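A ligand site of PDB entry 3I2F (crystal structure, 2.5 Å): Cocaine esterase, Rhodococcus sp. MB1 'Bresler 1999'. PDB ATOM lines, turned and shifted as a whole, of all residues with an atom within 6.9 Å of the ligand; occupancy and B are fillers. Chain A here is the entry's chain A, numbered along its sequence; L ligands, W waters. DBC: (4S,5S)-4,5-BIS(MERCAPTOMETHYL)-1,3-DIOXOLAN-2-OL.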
ATOM      1  N   PRO A  43      21.689   3.509   2.111  1.00  0.00           N
ATOM      2  CA  PRO A  43      21.355   4.816   1.519  1.00  0.00           C
ATOM      3  C   PRO A  43      19.855   5.063   1.317  1.00  0.00           C
ATOM      4  O   PRO A  43      19.493   6.147   0.851  1.00  0.00           O
ATOM      5  CB  PRO A  43      22.051   4.770   0.158  1.00  0.00           C
ATOM      6  CG  PRO A  43      22.029   3.355  -0.218  1.00  0.00           C
ATOM      7  CD  PRO A  43      22.112   2.548   1.071  1.00  0.00           C
ATOM      8  N   TYR A  44      19.013   4.086   1.631  1.00  0.00           N
ATOM      9  CA  TYR A  44      17.583   4.120   1.318  1.00  0.00           C
ATOM     10  C   TYR A  44      16.681   4.171   2.549  1.00  0.00           C
ATOM     11  O   TYR A  44      15.581   3.600   2.557  1.00  0.00           O
ATOM     12  CB  TYR A  44      17.201   2.917   0.424  1.00  0.00           C
ATOM     13  CG  TYR A  44      18.150   2.672  -0.735  1.00  0.00           C
ATOM     14  CD1 TYR A  44      18.303   3.618  -1.748  1.00  0.00           C
ATOM     15  CD2 TYR A  44      18.880   1.485  -0.827  1.00  0.00           C
ATOM     16  CE1 TYR A  44      19.175   3.398  -2.819  1.00  0.00           C
ATOM     17  CE2 TYR A  44      19.769   1.248  -1.896  1.00  0.00           C
ATOM     18  CZ  TYR A  44      19.908   2.210  -2.897  1.00  0.00           C
ATOM     19  OH  TYR A  44      20.771   2.004  -3.979  1.00  0.00           O
ATOM     20  N   GLN A  55      14.866  -8.836  -0.478  1.00  0.00           N
ATOM     21  CA  GLN A  55      15.937  -9.258  -1.399  1.00  0.00           C
ATOM     22  C   GLN A  55      17.095  -9.953  -0.653  1.00  0.00           C
ATOM     23  O   GLN A  55      18.011 -10.494  -1.296  1.00  0.00           O
ATOM     24  CB  GLN A  55      16.464  -8.053  -2.191  1.00  0.00           C
ATOM     25  CG  GLN A  55      15.420  -7.308  -3.027  1.00  0.00           C
ATOM     26  CD  GLN A  55      15.611  -5.799  -3.009  1.00  0.00           C
ATOM     27  OE1 GLN A  55      16.657  -5.287  -3.425  1.00  0.00           O
ATOM     28  NE2 GLN A  55      14.618  -5.089  -2.520  1.00  0.00           N
ATOM     29  N   HIS A  87      29.799   6.626  -2.584  1.00  0.00           N
ATOM     30  CA  HIS A  87      31.025   5.798  -2.520  1.00  0.00           C
ATOM     31  C   HIS A  87      32.217   6.398  -1.757  1.00  0.00           C
ATOM     32  O   HIS A  87      32.891   5.689  -0.999  1.00  0.00           O
ATOM     33  CB  HIS A  87      31.489   5.313  -3.922  1.00  0.00           C
ATOM     34  CG  HIS A  87      30.413   4.660  -4.749  1.00  0.00           C
ATOM     35  ND1 HIS A  87      29.498   3.757  -4.233  1.00  0.00           N
ATOM     36  CD2 HIS A  87      30.134   4.744  -6.077  1.00  0.00           C
ATOM     37  CE1 HIS A  87      28.693   3.346  -5.194  1.00  0.00           C
ATOM     38  NE2 HIS A  87      29.065   3.919  -6.328  1.00  0.00           N
ATOM     39  N   VAL A 116      22.178  -6.198   0.444  1.00  0.00           N
ATOM     40  CA  VAL A 116      22.104  -6.341  -1.001  1.00  0.00           C
ATOM     41  C   VAL A 116      22.471  -5.023  -1.675  1.00  0.00           C
ATOM     42  O   VAL A 116      22.232  -3.938  -1.125  1.00  0.00           O
ATOM     43  CB  VAL A 116      20.696  -6.830  -1.449  1.00  0.00           C
ATOM     44  CG1 VAL A 116      19.603  -5.784  -1.117  1.00  0.00           C
ATOM     45  CG2 VAL A 116      20.677  -7.189  -2.929  1.00  0.00           C
ATOM     46  N   SER A 117      23.090  -5.137  -2.855  1.00  0.00           N
ATOM     47  CA  SER A 117      23.342  -4.005  -3.737  1.00  0.00           C
ATOM     48  C   SER A 117      24.289  -2.984  -3.092  1.00  0.00           C
ATOM     49  O   SER A 117      25.450  -3.328  -2.805  1.00  0.00           O
ATOM     50  CB  SER A 117      22.012  -3.373  -4.174  1.00  0.00           C
ATOM     51  OG  SER A 117      22.187  -2.550  -5.307  1.00  0.00           O
ATOM     52  N   TYR A 118      23.806  -1.766  -2.819  1.00  0.00           N
ATOM     53  CA  TYR A 118      24.601  -0.747  -2.121  1.00  0.00           C
ATOM     54  C   TYR A 118      24.980  -1.207  -0.707  1.00  0.00           C
ATOM     55  O   TYR A 118      26.066  -0.907  -0.216  1.00  0.00           O
ATOM     56  CB  TYR A 118      23.848   0.585  -2.076  1.00  0.00           C
ATOM     57  CG  TYR A 118      24.728   1.833  -1.928  1.00  0.00           C
ATOM     58  CD1 TYR A 118      25.252   2.200  -0.679  1.00  0.00           C
ATOM     59  CD2 TYR A 118      25.004   2.641  -3.029  1.00  0.00           C
ATOM     60  CE1 TYR A 118      26.038   3.354  -0.530  1.00  0.00           C
ATOM     61  CE2 TYR A 118      25.795   3.806  -2.888  1.00  0.00           C
ATOM     62  CZ  TYR A 118      26.315   4.150  -1.648  1.00  0.00           C
ATOM     63  OH  TYR A 118      27.098   5.300  -1.521  1.00  0.00           O
ATOM     64  N   LEU A 119      24.089  -1.963  -0.074  1.00  0.00           N
ATOM     65  CA  LEU A 119      24.346  -2.561   1.234  1.00  0.00           C
ATOM     66  C   LEU A 119      25.360  -3.710   1.110  1.00  0.00           C
ATOM     67  O   LEU A 119      25.868  -4.195   2.115  1.00  0.00           O
ATOM     68  CB  LEU A 119      23.045  -3.046   1.887  1.00  0.00           C
ATOM     69  CG  LEU A 119      21.917  -2.051   2.216  1.00  0.00           C
ATOM     70  CD1 LEU A 119      21.503  -1.145   1.043  1.00  0.00           C
ATOM     71  CD2 LEU A 119      20.702  -2.807   2.727  1.00  0.00           C
ATOM     72  N   GLY A 120      25.647  -4.122  -0.123  1.00  0.00           N
ATOM     73  CA  GLY A 120      26.674  -5.115  -0.412  1.00  0.00           C
ATOM     74  C   GLY A 120      28.014  -4.475  -0.753  1.00  0.00           C
ATOM     75  O   GLY A 120      29.054  -4.963  -0.331  1.00  0.00           O
ATOM     76  N   VAL A 121      27.990  -3.397  -1.540  1.00  0.00           N
ATOM     77  CA  VAL A 121      29.200  -2.678  -1.936  1.00  0.00           C
ATOM     78  C   VAL A 121      29.906  -2.085  -0.705  1.00  0.00           C
ATOM     79  O   VAL A 121      31.140  -2.097  -0.596  1.00  0.00           O
ATOM     80  CB  VAL A 121      28.893  -1.547  -2.968  1.00  0.00           C
ATOM     81  CG1 VAL A 121      30.136  -0.709  -3.251  1.00  0.00           C
ATOM     82  CG2 VAL A 121      28.327  -2.141  -4.264  1.00  0.00           C
ATOM     83  N   MET A 141      24.536  -9.323  -4.391  1.00  0.00           N
ATOM     84  CA  MET A 141      24.444  -8.578  -5.683  1.00  0.00           C
ATOM     85  C   MET A 141      25.318  -7.289  -5.690  1.00  0.00           C
ATOM     86  O   MET A 141      24.792  -6.196  -5.938  1.00  0.00           O
ATOM     87  CB  MET A 141      22.953  -8.351  -6.131  1.00  0.00           C
ATOM     88  CG  MET A 141      22.253  -9.584  -6.727  1.00  0.00           C
ATOM     89  SD  MET A 141      20.469  -9.455  -6.538  1.00  0.00           S
ATOM     90  CE  MET A 141      19.884 -10.381  -7.962  1.00  0.00           C
ATOM     91  N   LEU A 146      33.875  -0.377  -8.813  1.00  0.00           N
ATOM     92  CA  LEU A 146      32.699   0.369  -9.249  1.00  0.00           C
ATOM     93  C   LEU A 146      32.692   0.700 -10.740  1.00  0.00           C
ATOM     94  O   LEU A 146      31.625   0.847 -11.348  1.00  0.00           O
ATOM     95  CB  LEU A 146      32.479   1.627  -8.401  1.00  0.00           C
ATOM     96  CG  LEU A 146      32.000   1.476  -6.953  1.00  0.00           C
ATOM     97  CD1 LEU A 146      30.761   0.562  -6.839  1.00  0.00           C
ATOM     98  CD2 LEU A 146      33.120   0.974  -6.091  1.00  0.00           C
ATOM     99  N   ALA A 149      31.511  -2.621 -12.317  1.00  0.00           N
ATOM    100  CA  ALA A 149      30.075  -2.697 -12.001  1.00  0.00           C
ATOM    101  C   ALA A 149      29.700  -1.726 -10.877  1.00  0.00           C
ATOM    102  O   ALA A 149      30.374  -1.670  -9.849  1.00  0.00           O
ATOM    103  CB  ALA A 149      29.672  -4.123 -11.636  1.00  0.00           C
ATOM    104  N   PRO A 150      28.617  -0.946 -11.070  1.00  0.00           N
ATOM    105  CA  PRO A 150      27.676  -0.952 -12.179  1.00  0.00           C
ATOM    106  C   PRO A 150      27.849   0.151 -13.220  1.00  0.00           C
ATOM    107  O   PRO A 150      27.053   0.209 -14.154  1.00  0.00           O
ATOM    108  CB  PRO A 150      26.351  -0.721 -11.460  1.00  0.00           C
ATOM    109  CG  PRO A 150      26.705   0.159 -10.267  1.00  0.00           C
ATOM    110  CD  PRO A 150      28.199   0.027 -10.038  1.00  0.00           C
ATOM    111  N   TRP A 151      28.851   1.026 -13.086  1.00  0.00           N
ATOM    112  CA  TRP A 151      28.846   2.267 -13.892  1.00  0.00           C
ATOM    113  C   TRP A 151      29.350   2.113 -15.325  1.00  0.00           C
ATOM    114  O   TRP A 151      28.742   2.640 -16.256  1.00  0.00           O
ATOM    115  CB  TRP A 151      29.494   3.438 -13.143  1.00  0.00           C
ATOM    116  CG  TRP A 151      28.939   3.595 -11.741  1.00  0.00           C
ATOM    117  CD1 TRP A 151      29.666   3.646 -10.581  1.00  0.00           C
ATOM    118  CD2 TRP A 151      27.562   3.687 -11.359  1.00  0.00           C
ATOM    119  NE1 TRP A 151      28.821   3.781  -9.495  1.00  0.00           N
ATOM    120  CE2 TRP A 151      27.522   3.795  -9.946  1.00  0.00           C
ATOM    121  CE3 TRP A 151      26.349   3.672 -12.069  1.00  0.00           C
ATOM    122  CZ2 TRP A 151      26.322   3.903  -9.227  1.00  0.00           C
ATOM    123  CZ3 TRP A 151      25.149   3.781 -11.350  1.00  0.00           C
ATOM    124  CH2 TRP A 151      25.150   3.889  -9.948  1.00  0.00           C
ATOM    125  N   ALA A 162      21.748   2.302 -16.166  1.00  0.00           N
ATOM    126  CA  ALA A 162      22.006   2.138 -14.731  1.00  0.00           C
ATOM    127  C   ALA A 162      22.242   3.512 -14.099  1.00  0.00           C
ATOM    128  O   ALA A 162      21.643   3.828 -13.066  1.00  0.00           O
ATOM    129  CB  ALA A 162      23.196   1.225 -14.482  1.00  0.00           C
ATOM    130  N   LEU A 163      23.076   4.326 -14.741  1.00  0.00           N
ATOM    131  CA  LEU A 163      23.425   5.643 -14.246  1.00  0.00           C
ATOM    132  C   LEU A 163      22.224   6.603 -14.107  1.00  0.00           C
ATOM    133  O   LEU A 163      22.028   7.186 -13.057  1.00  0.00           O
ATOM    134  CB  LEU A 163      24.508   6.276 -15.123  1.00  0.00           C
ATOM    135  CG  LEU A 163      24.879   7.703 -14.682  1.00  0.00           C
ATOM    136  CD1 LEU A 163      25.567   7.699 -13.297  1.00  0.00           C
ATOM    137  CD2 LEU A 163      25.727   8.379 -15.707  1.00  0.00           C
ATOM    138  N   GLY A 165      18.925   5.843 -14.215  1.00  0.00           N
ATOM    139  CA  GLY A 165      17.873   5.269 -13.391  1.00  0.00           C
ATOM    140  C   GLY A 165      18.206   5.455 -11.935  1.00  0.00           C
ATOM    141  O   GLY A 165      17.379   5.957 -11.157  1.00  0.00           O
ATOM    142  N   TRP A 166      19.419   5.089 -11.553  1.00  0.00           N
ATOM    143  CA  TRP A 166      19.820   5.204 -10.165  1.00  0.00           C
ATOM    144  C   TRP A 166      19.821   6.670  -9.692  1.00  0.00           C
ATOM    145  O   TRP A 166      19.287   6.979  -8.625  1.00  0.00           O
ATOM    146  CB  TRP A 166      21.171   4.559  -9.903  1.00  0.00           C
ATOM    147  CG  TRP A 166      21.472   4.442  -8.437  1.00  0.00           C
ATOM    148  CD1 TRP A 166      20.806   3.666  -7.512  1.00  0.00           C
ATOM    149  CD2 TRP A 166      22.497   5.141  -7.710  1.00  0.00           C
ATOM    150  NE1 TRP A 166      21.365   3.831  -6.261  1.00  0.00           N
ATOM    151  CE2 TRP A 166      22.410   4.719  -6.357  1.00  0.00           C
ATOM    152  CE3 TRP A 166      23.494   6.060  -8.070  1.00  0.00           C
ATOM    153  CZ2 TRP A 166      23.258   5.208  -5.363  1.00  0.00           C
ATOM    154  CZ3 TRP A 166      24.343   6.537  -7.092  1.00  0.00           C
ATOM    155  CH2 TRP A 166      24.213   6.108  -5.750  1.00  0.00           C
ATOM    156  N   LEU A 169      16.551   7.879  -8.950  1.00  0.00           N
ATOM    157  CA  LEU A 169      16.060   7.275  -7.715  1.00  0.00           C
ATOM    158  C   LEU A 169      16.590   8.011  -6.478  1.00  0.00           C
ATOM    159  O   LEU A 169      15.854   8.288  -5.539  1.00  0.00           O
ATOM    160  CB  LEU A 169      16.441   5.801  -7.657  1.00  0.00           C
ATOM    161  CG  LEU A 169      15.768   5.022  -6.517  1.00  0.00           C
ATOM    162  CD1 LEU A 169      14.421   4.439  -7.005  1.00  0.00           C
ATOM    163  CD2 LEU A 169      16.705   3.930  -5.942  1.00  0.00           C
ATOM    164  N   PHE A 261      25.495  -6.852 -11.520  1.00  0.00           N
ATOM    165  CA  PHE A 261      26.745  -7.034 -10.786  1.00  0.00           C
ATOM    166  C   PHE A 261      27.372  -8.442 -10.946  1.00  0.00           C
ATOM    167  O   PHE A 261      28.466  -8.696 -10.406  1.00  0.00           O
ATOM    168  CB  PHE A 261      26.525  -6.754  -9.290  1.00  0.00           C
ATOM    169  CG  PHE A 261      26.258  -5.296  -8.954  1.00  0.00           C
ATOM    170  CD1 PHE A 261      24.954  -4.796  -8.956  1.00  0.00           C
ATOM    171  CD2 PHE A 261      27.291  -4.453  -8.582  1.00  0.00           C
ATOM    172  CE1 PHE A 261      24.696  -3.449  -8.625  1.00  0.00           C
ATOM    173  CE2 PHE A 261      27.059  -3.114  -8.244  1.00  0.00           C
ATOM    174  CZ  PHE A 261      25.758  -2.601  -8.267  1.00  0.00           C
ATOM    175  N   HIS A 287      18.274  -7.589 -10.977  1.00  0.00           N
ATOM    176  CA  HIS A 287      18.408  -6.758  -9.776  1.00  0.00           C
ATOM    177  C   HIS A 287      17.070  -6.449  -9.128  1.00  0.00           C
ATOM    178  O   HIS A 287      16.991  -6.386  -7.922  1.00  0.00           O
ATOM    179  CB  HIS A 287      19.151  -5.461 -10.072  1.00  0.00           C
ATOM    180  CG  HIS A 287      19.937  -4.942  -8.905  1.00  0.00           C
ATOM    181  ND1 HIS A 287      21.046  -5.588  -8.398  1.00  0.00           N
ATOM    182  CD2 HIS A 287      19.773  -3.821  -8.151  1.00  0.00           C
ATOM    183  CE1 HIS A 287      21.531  -4.893  -7.395  1.00  0.00           C
ATOM    184  NE2 HIS A 287      20.781  -3.829  -7.214  1.00  0.00           N
ATOM    185  N   LEU A 407      19.359  -2.906 -15.573  1.00  0.00           N
ATOM    186  CA  LEU A 407      19.078  -2.554 -14.172  1.00  0.00           C
ATOM    187  C   LEU A 407      17.767  -1.769 -13.998  1.00  0.00           C
ATOM    188  O   LEU A 407      16.902  -2.177 -13.222  1.00  0.00           O
ATOM    189  CB  LEU A 407      20.280  -1.823 -13.531  1.00  0.00           C
ATOM    190  CG  LEU A 407      21.465  -2.743 -13.164  1.00  0.00           C
ATOM    191  CD1 LEU A 407      22.746  -1.989 -12.871  1.00  0.00           C
ATOM    192  CD2 LEU A 407      21.157  -3.616 -11.980  1.00  0.00           C
ATOM    193  N   PHE A 408      17.604  -0.672 -14.734  1.00  0.00           N
ATOM    194  CA  PHE A 408      16.434   0.200 -14.515  1.00  0.00           C
ATOM    195  C   PHE A 408      15.489   0.268 -15.704  1.00  0.00           C
ATOM    196  O   PHE A 408      14.275   0.333 -15.527  1.00  0.00           O
ATOM    197  CB  PHE A 408      16.867   1.609 -14.069  1.00  0.00           C
ATOM    198  CG  PHE A 408      17.424   1.640 -12.670  1.00  0.00           C
ATOM    199  CD1 PHE A 408      16.569   1.826 -11.585  1.00  0.00           C
ATOM    200  CD2 PHE A 408      18.775   1.451 -12.446  1.00  0.00           C
ATOM    201  CE1 PHE A 408      17.083   1.835 -10.271  1.00  0.00           C
ATOM    202  CE2 PHE A 408      19.290   1.448 -11.149  1.00  0.00           C
ATOM    203  CZ  PHE A 408      18.444   1.637 -10.066  1.00  0.00           C
HETATM  204  O4  DBC L   1      21.274  -0.595  -4.027  1.00  0.00           O
HETATM  205  C5  DBC L   1      21.828  -1.018  -5.307  1.00  0.00           C
HETATM  206  O3  DBC L   1      21.078  -0.635  -6.553  1.00  0.00           O
HETATM  207  O2  DBC L   1      23.167  -0.458  -5.502  1.00  0.00           O
HETATM  208  C2  DBC L   1      23.349  -0.121  -6.872  1.00  0.00           C
HETATM  209  C1  DBC L   1      24.234   1.115  -6.976  1.00  0.00           C
HETATM  210  S1  DBC L   1      25.913   0.880  -6.334  1.00  0.00           S
HETATM  211  C3  DBC L   1      21.944   0.091  -7.403  1.00  0.00           C
HETATM  212  C4  DBC L   1      21.787  -0.412  -8.823  1.00  0.00           C
HETATM  213  S4  DBC L   1      22.668   0.671  -9.973  1.00  0.00           S
HETATM  214  O   HOH W   1      18.681  -1.402  -4.100  1.00  0.00           O
HETATM  215  O   HOH W   2      18.374   0.141  -6.348  1.00  0.00           O
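A ring nitrogen (NE2) of His 287 is in hydrogen-bond range of the side-chain hydroxyl (OG) of Ser 117, at 2.7 Å.
NE1 of Trp 166 is in hydrogen-bond range of OH of Tyr 44.
The side-chain hydroxyl of Tyr 118 sits at hydrogen-bond distance from the backbone NH of His 87 (3.2 Å).
NE1 of Trp 151 sits at hydrogen-bond distance from NE2 of His 87 (3.2 Å).
Residues that only touch the ligand: His 87 (3.9 Å), Trp 166 (3.8 Å), Phe 261 (3.7 Å), Leu 407 (3.9 Å) and Phe 408 (3.7 Å).
Hydrophobic or aromatic side chains that line the ligand: Tyr 44, His 87, Tyr 118, Trp 166, Phe 261, His 287, Leu 407 and Phe 408.
OG of Ser 117 is covalently linked to C5 of the ligand, at 1.6 Å.
An oxygen (O4) of the ligand sits at hydrogen-bond distance from the side-chain hydroxyl (OH) of Tyr 44 (2.6 Å).
N of Tyr 118 is in hydrogen-bond range of O4 of the ligand (3.0 Å).
NE2 of His 287 is in hydrogen-bond range of O3 of the ligand, 3.3 Å away.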
